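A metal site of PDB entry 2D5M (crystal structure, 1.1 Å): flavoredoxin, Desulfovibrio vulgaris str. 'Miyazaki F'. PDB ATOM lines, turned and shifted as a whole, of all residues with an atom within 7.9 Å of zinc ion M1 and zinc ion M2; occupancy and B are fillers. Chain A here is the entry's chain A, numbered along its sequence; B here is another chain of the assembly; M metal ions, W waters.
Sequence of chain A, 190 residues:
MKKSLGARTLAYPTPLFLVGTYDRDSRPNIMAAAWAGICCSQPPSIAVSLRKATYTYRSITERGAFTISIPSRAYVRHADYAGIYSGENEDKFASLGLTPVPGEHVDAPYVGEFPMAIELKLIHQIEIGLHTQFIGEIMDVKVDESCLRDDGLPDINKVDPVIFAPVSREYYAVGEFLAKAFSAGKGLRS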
ATOM      1  N   GLY A  37     -18.319 -33.730  -3.751  1.00  0.00           N
ATOM      2  CA  GLY A  37     -19.145 -33.016  -2.797  1.00  0.00           C
ATOM      3  C   GLY A  37     -20.120 -32.152  -3.540  1.00  0.00           C
ATOM      4  O   GLY A  37     -20.130 -32.062  -4.751  1.00  0.00           O
ATOM      5  N   ILE A  38     -21.064 -31.552  -2.773  1.00  0.00           N
ATOM      6  CA  ILE A  38     -22.009 -30.600  -3.359  1.00  0.00           C
ATOM      7  C   ILE A  38     -21.218 -29.397  -3.829  1.00  0.00           C
ATOM      8  O   ILE A  38     -20.312 -28.938  -3.115  1.00  0.00           O
ATOM      9  CB  ILE A  38     -23.109 -30.262  -2.375  1.00  0.00           C
ATOM     10  CG1 ILE A  38     -23.908 -31.527  -1.989  1.00  0.00           C
ATOM     11  CG2 ILE A  38     -24.013 -29.154  -2.891  1.00  0.00           C
ATOM     12  CD1 ILE A  38     -24.857 -31.345  -0.830  1.00  0.00           C
ATOM     13  N   CYS A  39     -21.527 -28.886  -5.007  1.00  0.00           N
ATOM     14  CA  CYS A  39     -20.831 -27.707  -5.513  1.00  0.00           C
ATOM     15  C   CYS A  39     -21.703 -26.503  -5.657  1.00  0.00           C
ATOM     16  O   CYS A  39     -21.165 -25.382  -5.599  1.00  0.00           O
ATOM     17  CB  CYS A  39     -20.086 -27.932  -6.833  1.00  0.00           C
ATOM     18  SG  CYS A  39     -21.153 -28.470  -8.216  1.00  0.00           S
ATOM     19  N   CYS A  40     -22.987 -26.625  -5.871  1.00  0.00           N
ATOM     20  CA  CYS A  40     -23.839 -25.475  -6.128  1.00  0.00           C
ATOM     21  C   CYS A  40     -25.232 -25.735  -5.593  1.00  0.00           C
ATOM     22  O   CYS A  40     -25.722 -26.853  -5.567  1.00  0.00           O
ATOM     23  CB  CYS A  40     -24.059 -25.093  -7.609  1.00  0.00           C
ATOM     24  SG  CYS A  40     -22.580 -24.544  -8.445  1.00  0.00           S
ATOM     25  N   SER A  41     -25.899 -24.635  -5.228  1.00  0.00           N
ATOM     26  CA  SER A  41     -27.285 -24.651  -4.868  1.00  0.00           C
ATOM     27  C   SER A  41     -28.222 -24.283  -6.013  1.00  0.00           C
ATOM     28  O   SER A  41     -29.421 -24.501  -5.902  1.00  0.00           O
ATOM     29  CB  SER A  41     -27.563 -23.739  -3.673  1.00  0.00           C
ATOM     30  OG  SER A  41     -26.861 -24.305  -2.589  1.00  0.00           O
ATOM     31  N   GLN A  42     -27.713 -23.685  -7.100  1.00  0.00           N
ATOM     32  CA  GLN A  42     -28.553 -23.367  -8.244  1.00  0.00           C
ATOM     33  C   GLN A  42     -27.839 -23.698  -9.541  1.00  0.00           C
ATOM     34  O   GLN A  42     -26.939 -22.960  -9.870  1.00  0.00           O
ATOM     35  CB  GLN A  42     -28.989 -21.894  -8.293  1.00  0.00           C
ATOM     36  CG  GLN A  42     -30.060 -21.697  -9.375  1.00  0.00           C
ATOM     37  CD  GLN A  42     -31.368 -22.309  -8.965  1.00  0.00           C
ATOM     38  OE1 GLN A  42     -32.263 -21.687  -8.339  1.00  0.00           O
ATOM     39  NE2 GLN A  42     -31.578 -23.498  -9.259  1.00  0.00           N
ATOM     40  N   PRO A  43     -28.208 -24.734 -10.262  1.00  0.00           N
ATOM     41  CA  PRO A  43     -29.101 -25.819  -9.799  1.00  0.00           C
ATOM     42  C   PRO A  43     -28.394 -26.593  -8.727  1.00  0.00           C
ATOM     43  O   PRO A  43     -27.151 -26.582  -8.695  1.00  0.00           O
ATOM     44  CB  PRO A  43     -29.371 -26.651 -11.057  1.00  0.00           C
ATOM     45  CG  PRO A  43     -28.175 -26.425 -11.884  1.00  0.00           C
ATOM     46  CD  PRO A  43     -27.634 -25.044 -11.594  1.00  0.00           C
ATOM     47  N   PRO A  44     -29.159 -27.328  -7.952  1.00  0.00           N
ATOM     48  CA  PRO A  44     -28.500 -28.185  -6.939  1.00  0.00           C
ATOM     49  C   PRO A  44     -27.593 -29.148  -7.695  1.00  0.00           C
ATOM     50  O   PRO A  44     -28.071 -29.792  -8.638  1.00  0.00           O
ATOM     51  CB  PRO A  44     -29.680 -28.887  -6.267  1.00  0.00           C
ATOM     52  CG  PRO A  44     -30.799 -28.779  -7.302  1.00  0.00           C
ATOM     53  CD  PRO A  44     -30.591 -27.480  -8.005  1.00  0.00           C
ATOM     54  N   SER A  45     -26.329 -29.239  -7.329  1.00  0.00           N
ATOM     55  CA  SER A  45     -25.336 -29.976  -8.095  1.00  0.00           C
ATOM     56  C   SER A  45     -24.291 -30.619  -7.221  1.00  0.00           C
ATOM     57  O   SER A  45     -23.962 -30.078  -6.151  1.00  0.00           O
ATOM     58  CB  SER A  45     -24.588 -29.028  -9.058  1.00  0.00           C
ATOM     59  OG  SER A  45     -25.394 -28.314  -9.955  1.00  0.00           O
ATOM     60  N   ILE A  46     -23.749 -31.737  -7.694  1.00  0.00           N
ATOM     61  CA  ILE A  46     -22.625 -32.425  -7.090  1.00  0.00           C
ATOM     62  C   ILE A  46     -21.513 -32.530  -8.106  1.00  0.00           C
ATOM     63  O   ILE A  46     -21.764 -32.871  -9.275  1.00  0.00           O
ATOM     64  CB  ILE A  46     -23.046 -33.833  -6.556  1.00  0.00           C
ATOM     65  CG1 ILE A  46     -23.976 -33.607  -5.362  1.00  0.00           C
ATOM     66  CG2 ILE A  46     -21.848 -34.692  -6.218  1.00  0.00           C
ATOM     67  CD1 ILE A  46     -24.643 -34.894  -4.855  1.00  0.00           C
ATOM     68  N   ALA A  47     -20.316 -32.281  -7.654  1.00  0.00           N
ATOM     69  CA  ALA A  47     -19.072 -32.457  -8.423  1.00  0.00           C
ATOM     70  C   ALA A  47     -18.403 -33.752  -7.994  1.00  0.00           C
ATOM     71  O   ALA A  47     -18.282 -34.044  -6.808  1.00  0.00           O
ATOM     72  CB  ALA A  47     -18.169 -31.267  -8.194  1.00  0.00           C
ATOM     73  N   ILE A 123     -24.125 -31.801 -16.409  1.00  0.00           N
ATOM     74  CA  ILE A 123     -24.269 -30.420 -16.891  1.00  0.00           C
ATOM     75  C   ILE A 123     -22.912 -29.772 -17.194  1.00  0.00           C
ATOM     76  O   ILE A 123     -22.900 -28.829 -18.012  1.00  0.00           O
ATOM     77  CB  ILE A 123     -25.145 -29.556 -15.965  1.00  0.00           C
ATOM     78  CG1 ILE A 123     -24.617 -29.516 -14.527  1.00  0.00           C
ATOM     79  CG2 ILE A 123     -26.582 -30.013 -16.044  1.00  0.00           C
ATOM     80  CD1 ILE A 123     -25.216 -28.361 -13.735  1.00  0.00           C
ATOM     81  N   HIS A 124     -21.798 -30.221 -16.642  1.00  0.00           N
ATOM     82  CA  HIS A 124     -20.518 -29.655 -17.017  1.00  0.00           C
ATOM     83  C   HIS A 124     -19.481 -30.738 -16.938  1.00  0.00           C
ATOM     84  O   HIS A 124     -19.566 -31.640 -16.072  1.00  0.00           O
ATOM     85  CB  HIS A 124     -20.050 -28.512 -16.104  1.00  0.00           C
ATOM     86  CG  HIS A 124     -20.997 -27.360 -15.915  1.00  0.00           C
ATOM     87  ND1 HIS A 124     -21.253 -26.432 -16.908  1.00  0.00           N
ATOM     88  CD2 HIS A 124     -21.733 -26.977 -14.826  1.00  0.00           C
ATOM     89  CE1 HIS A 124     -22.119 -25.539 -16.431  1.00  0.00           C
ATOM     90  NE2 HIS A 124     -22.430 -25.836 -15.185  1.00  0.00           N
ATOM     91  N   ILE A 126     -15.492 -30.500 -16.577  1.00  0.00           N
ATOM     92  CA  ILE A 126     -14.454 -29.486 -16.347  1.00  0.00           C
ATOM     93  C   ILE A 126     -13.097 -30.122 -16.425  1.00  0.00           C
ATOM     94  O   ILE A 126     -12.808 -31.116 -15.748  1.00  0.00           O
ATOM     95  CB  ILE A 126     -14.654 -28.800 -15.006  1.00  0.00           C
ATOM     96  CG1 ILE A 126     -16.038 -28.098 -14.957  1.00  0.00           C
ATOM     97  CG2 ILE A 126     -13.582 -27.835 -14.567  1.00  0.00           C
ATOM     98  CD1 ILE A 126     -16.506 -27.666 -13.623  1.00  0.00           C
ATOM     99  N   GLN A 133     -13.384 -32.891 -13.503  1.00  0.00           N
ATOM    100  CA  GLN A 133     -14.558 -33.079 -12.675  1.00  0.00           C
ATOM    101  C   GLN A 133     -15.786 -33.129 -13.549  1.00  0.00           C
ATOM    102  O   GLN A 133     -15.957 -32.350 -14.478  1.00  0.00           O
ATOM    103  CB  GLN A 133     -14.832 -31.995 -11.579  1.00  0.00           C
ATOM    104  CG  GLN A 133     -13.791 -31.662 -10.574  1.00  0.00           C
ATOM    105  CD  GLN A 133     -14.287 -30.268 -10.068  1.00  0.00           C
ATOM    106  OE1 GLN A 133     -14.814 -30.179  -8.985  1.00  0.00           O
ATOM    107  NE2 GLN A 133     -14.153 -29.344 -11.029  1.00  0.00           N
ATOM    108  N   ILE A 135     -19.785 -32.447 -13.295  1.00  0.00           N
ATOM    109  CA  ILE A 135     -20.770 -31.715 -12.493  1.00  0.00           C
ATOM    110  C   ILE A 135     -22.121 -32.248 -12.889  1.00  0.00           C
ATOM    111  O   ILE A 135     -22.550 -32.157 -14.068  1.00  0.00           O
ATOM    112  CB  ILE A 135     -20.710 -30.218 -12.732  1.00  0.00           C
ATOM    113  CG1 ILE A 135     -19.288 -29.648 -12.638  1.00  0.00           C
ATOM    114  CG2 ILE A 135     -21.683 -29.524 -11.800  1.00  0.00           C
ATOM    115  CD1 ILE A 135     -18.666 -29.893 -11.318  1.00  0.00           C
ATOM    116  N   GLY A 136     -22.821 -32.852 -11.939  1.00  0.00           N
ATOM    117  CA  GLY A 136     -24.164 -33.339 -12.149  1.00  0.00           C
ATOM    118  C   GLY A 136     -25.188 -32.466 -11.466  1.00  0.00           C
ATOM    119  O   GLY A 136     -25.019 -32.070 -10.328  1.00  0.00           O
ATOM    120  N   GLU A 137     -26.256 -32.166 -12.202  1.00  0.00           N
ATOM    121  CA  GLU A 137     -27.418 -31.504 -11.632  1.00  0.00           C
ATOM    122  C   GLU A 137     -28.260 -32.573 -10.946  1.00  0.00           C
ATOM    123  O   GLU A 137     -28.615 -33.588 -11.540  1.00  0.00           O
ATOM    124  CB  GLU A 137     -28.245 -30.815 -12.696  1.00  0.00           C
ATOM    125  CG  GLU A 137     -29.491 -30.165 -12.157  1.00  0.00           C
ATOM    126  CD  GLU A 137     -30.294 -29.346 -13.154  1.00  0.00           C
ATOM    127  OE1 GLU A 137     -29.779 -29.072 -14.269  1.00  0.00           O
ATOM    128  OE2 GLU A 137     -31.449 -28.960 -12.801  1.00  0.00           O
ATOM    129  N   TRP B  35     -19.884 -26.754   0.798  1.00  0.00           N
ATOM    130  CA  TRP B  35     -19.914 -27.098  -0.623  1.00  0.00           C
ATOM    131  C   TRP B  35     -18.456 -27.187  -1.062  1.00  0.00           C
ATOM    132  O   TRP B  35     -17.877 -26.286  -1.674  1.00  0.00           O
ATOM    133  CB  TRP B  35     -20.674 -26.077  -1.434  1.00  0.00           C
ATOM    134  CG  TRP B  35     -22.174 -26.074  -1.369  1.00  0.00           C
ATOM    135  CD1 TRP B  35     -22.917 -25.323  -2.222  1.00  0.00           C
ATOM    136  CD2 TRP B  35     -23.123 -26.759  -0.541  1.00  0.00           C
ATOM    137  NE1 TRP B  35     -24.249 -25.497  -1.979  1.00  0.00           N
ATOM    138  CE2 TRP B  35     -24.415 -26.369  -0.952  1.00  0.00           C
ATOM    139  CE3 TRP B  35     -23.033 -27.689   0.502  1.00  0.00           C
ATOM    140  CZ2 TRP B  35     -25.580 -26.847  -0.364  1.00  0.00           C
ATOM    141  CZ3 TRP B  35     -24.185 -28.161   1.108  1.00  0.00           C
ATOM    142  CH2 TRP B  35     -25.461 -27.743   0.670  1.00  0.00           C
ATOM    143  N   SER B  49     -16.674 -24.037  -3.099  1.00  0.00           N
ATOM    144  CA  SER B  49     -17.602 -23.160  -3.801  1.00  0.00           C
ATOM    145  C   SER B  49     -17.978 -22.009  -2.909  1.00  0.00           C
ATOM    146  O   SER B  49     -18.774 -22.223  -2.011  1.00  0.00           O
ATOM    147  CB  SER B  49     -18.836 -23.963  -4.199  1.00  0.00           C
ATOM    148  OG  SER B  49     -18.532 -24.963  -5.108  1.00  0.00           O
ATOM    149  N   LEU B  50     -17.432 -20.827  -3.136  1.00  0.00           N
ATOM    150  CA  LEU B  50     -17.668 -19.648  -2.335  1.00  0.00           C
ATOM    151  C   LEU B  50     -18.376 -18.596  -3.166  1.00  0.00           C
ATOM    152  O   LEU B  50     -17.934 -18.247  -4.256  1.00  0.00           O
ATOM    153  CB  LEU B  50     -16.336 -19.066  -1.814  1.00  0.00           C
ATOM    154  CG  LEU B  50     -15.431 -20.019  -1.013  1.00  0.00           C
ATOM    155  CD1 LEU B  50     -14.226 -19.342  -0.414  1.00  0.00           C
ATOM    156  CD2 LEU B  50     -16.264 -20.729   0.076  1.00  0.00           C
ATOM    157  N   ARG B  51     -19.446 -18.069  -2.628  1.00  0.00           N
ATOM    158  CA  ARG B  51     -20.228 -17.057  -3.292  1.00  0.00           C
ATOM    159  C   ARG B  51     -19.513 -15.726  -3.335  1.00  0.00           C
ATOM    160  O   ARG B  51     -18.810 -15.311  -2.431  1.00  0.00           O
ATOM    161  CB  ARG B  51     -21.587 -16.878  -2.575  1.00  0.00           C
ATOM    162  CG  ARG B  51     -22.501 -18.056  -2.742  1.00  0.00           C
ATOM    163  CD  ARG B  51     -23.772 -18.049  -1.847  1.00  0.00           C
ATOM    164  NE  ARG B  51     -23.227 -18.127  -0.506  1.00  0.00           N
ATOM    165  CZ  ARG B  51     -23.084 -17.124   0.373  1.00  0.00           C
ATOM    166  NH1 ARG B  51     -23.580 -15.923   0.184  1.00  0.00           N
ATOM    167  NH2 ARG B  51     -22.425 -17.397   1.488  1.00  0.00           N
ATOM    168  N   HIS B 131     -21.728 -22.022 -12.090  1.00  0.00           N
ATOM    169  CA  HIS B 131     -20.875 -22.791 -11.152  1.00  0.00           C
ATOM    170  C   HIS B 131     -19.607 -22.003 -10.873  1.00  0.00           C
ATOM    171  O   HIS B 131     -18.965 -21.616 -11.842  1.00  0.00           O
ATOM    172  CB  HIS B 131     -20.789 -24.105 -11.785  1.00  0.00           C
ATOM    173  CG  HIS B 131     -19.687 -24.928 -11.283  1.00  0.00           C
ATOM    174  ND1 HIS B 131     -20.004 -25.940 -10.428  1.00  0.00           N
ATOM    175  CD2 HIS B 131     -18.372 -24.964 -11.545  1.00  0.00           C
ATOM    176  CE1 HIS B 131     -18.855 -26.578 -10.148  1.00  0.00           C
ATOM    177  NE2 HIS B 131     -17.878 -25.983 -10.801  1.00  0.00           N
ATOM    178  N   THR B 132     -19.250 -21.804  -9.599  1.00  0.00           N
ATOM    179  CA  THR B 132     -18.063 -21.060  -9.147  1.00  0.00           C
ATOM    180  C   THR B 132     -17.266 -21.816  -8.097  1.00  0.00           C
ATOM    181  O   THR B 132     -17.832 -22.223  -7.079  1.00  0.00           O
ATOM    182  CB  THR B 132     -18.683 -19.699  -8.600  1.00  0.00           C
ATOM    183  OG1 THR B 132     -19.379 -19.052  -9.686  1.00  0.00           O
ATOM    184  CG2 THR B 132     -17.626 -18.849  -8.049  1.00  0.00           C
ATOM    185  N   GLN B 133     -15.990 -22.025  -8.297  1.00  0.00           N
ATOM    186  CA  GLN B 133     -15.212 -22.782  -7.347  1.00  0.00           C
ATOM    187  C   GLN B 133     -13.791 -22.270  -7.343  1.00  0.00           C
ATOM    188  O   GLN B 133     -13.189 -22.007  -8.376  1.00  0.00           O
ATOM    189  CB  GLN B 133     -15.124 -24.330  -7.567  1.00  0.00           C
ATOM    190  CG  GLN B 133     -16.369 -25.140  -7.677  1.00  0.00           C
ATOM    191  CD  GLN B 133     -15.825 -26.434  -8.367  1.00  0.00           C
ATOM    192  OE1 GLN B 133     -15.677 -27.444  -7.717  1.00  0.00           O
ATOM    193  NE2 GLN B 133     -15.470 -26.178  -9.628  1.00  0.00           N
HETATM  194 ZN    ZN M   1     -21.689 -26.450  -9.362  1.00  0.00          ZN
HETATM  195 ZN    ZN M   2     -23.035 -22.139  -7.097  1.00  0.00          ZN
HETATM  196  O   HOH W   1     -23.823 -20.453  -7.475  1.00  0.00           O
HETATM  197  O   HOH W   2     -24.158 -22.166  -4.442  1.00  0.00           O
HETATM  198  O   HOH W   3     -23.240 -26.734 -10.958  1.00  0.00           O
HETATM  199  O   HOH W   4     -20.739 -22.591  -6.907  1.00  0.00           O
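OG of Ser 45 is in hydrogen-bond range of O of Pro 43 (2.8 Å). The backbone NH of Ser 45 lies within hydrogen-bond range of the backbone carbonyl oxygen of Cys 40 (3.0 Å). O of Cys 39 lies within hydrogen-bond range of OG of Ser 49 of chain B, at 2.7 Å. O of Ser 45 is in hydrogen-bond range of N of Cys 39, 2.9 Å away. NE2 of Gln 133 of chain B lies within hydrogen-bond range of NE2 of His 131 of chain B, at 2.7 Å. O of Ile 135 lies within hydrogen-bond range of N of Ile 123 (2.8 Å). N of Ile 135 is in hydrogen-bond range of O of His 124, 2.9 Å away.
One residue has an atom within 4 Å of zinc ion M2: Cys 40. The nearest printed residue that does not touch zinc ion M2 is Cys 39 (4.03 Å).
Zinc ion M2 is bound by water W1 (1.9 Å), water W4 (2.3 Å) and the side-chain sulfur (SG) of Cys 40 (2.8 Å). Zinc ion M2 has three donor atoms within binding distance.
Water W4 bridges the backbone carbonyl oxygen of Thr 132 of chain B and the backbone carbonyl oxygen of Cys 39.
Zinc ion M1 is bound by a ring nitrogen (ND1) of His 131 of chain B (2.1 Å), water W3 (2.2 Å), the side-chain sulfur of Cys 40 (2.3 Å) and the side-chain sulfur of Cys 39 (2.4 Å). Zinc ion M1 has four donor atoms within binding distance.
Ser 45 touches zinc ion M1 (CB to ZN, 3.9 Å). Ile 135 touches zinc ion M1. Five residues have an atom within 4 Å of zinc ion M1: Cys 39, Cys 40, Ser 45, Ile 135 and His 131 of chain B.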
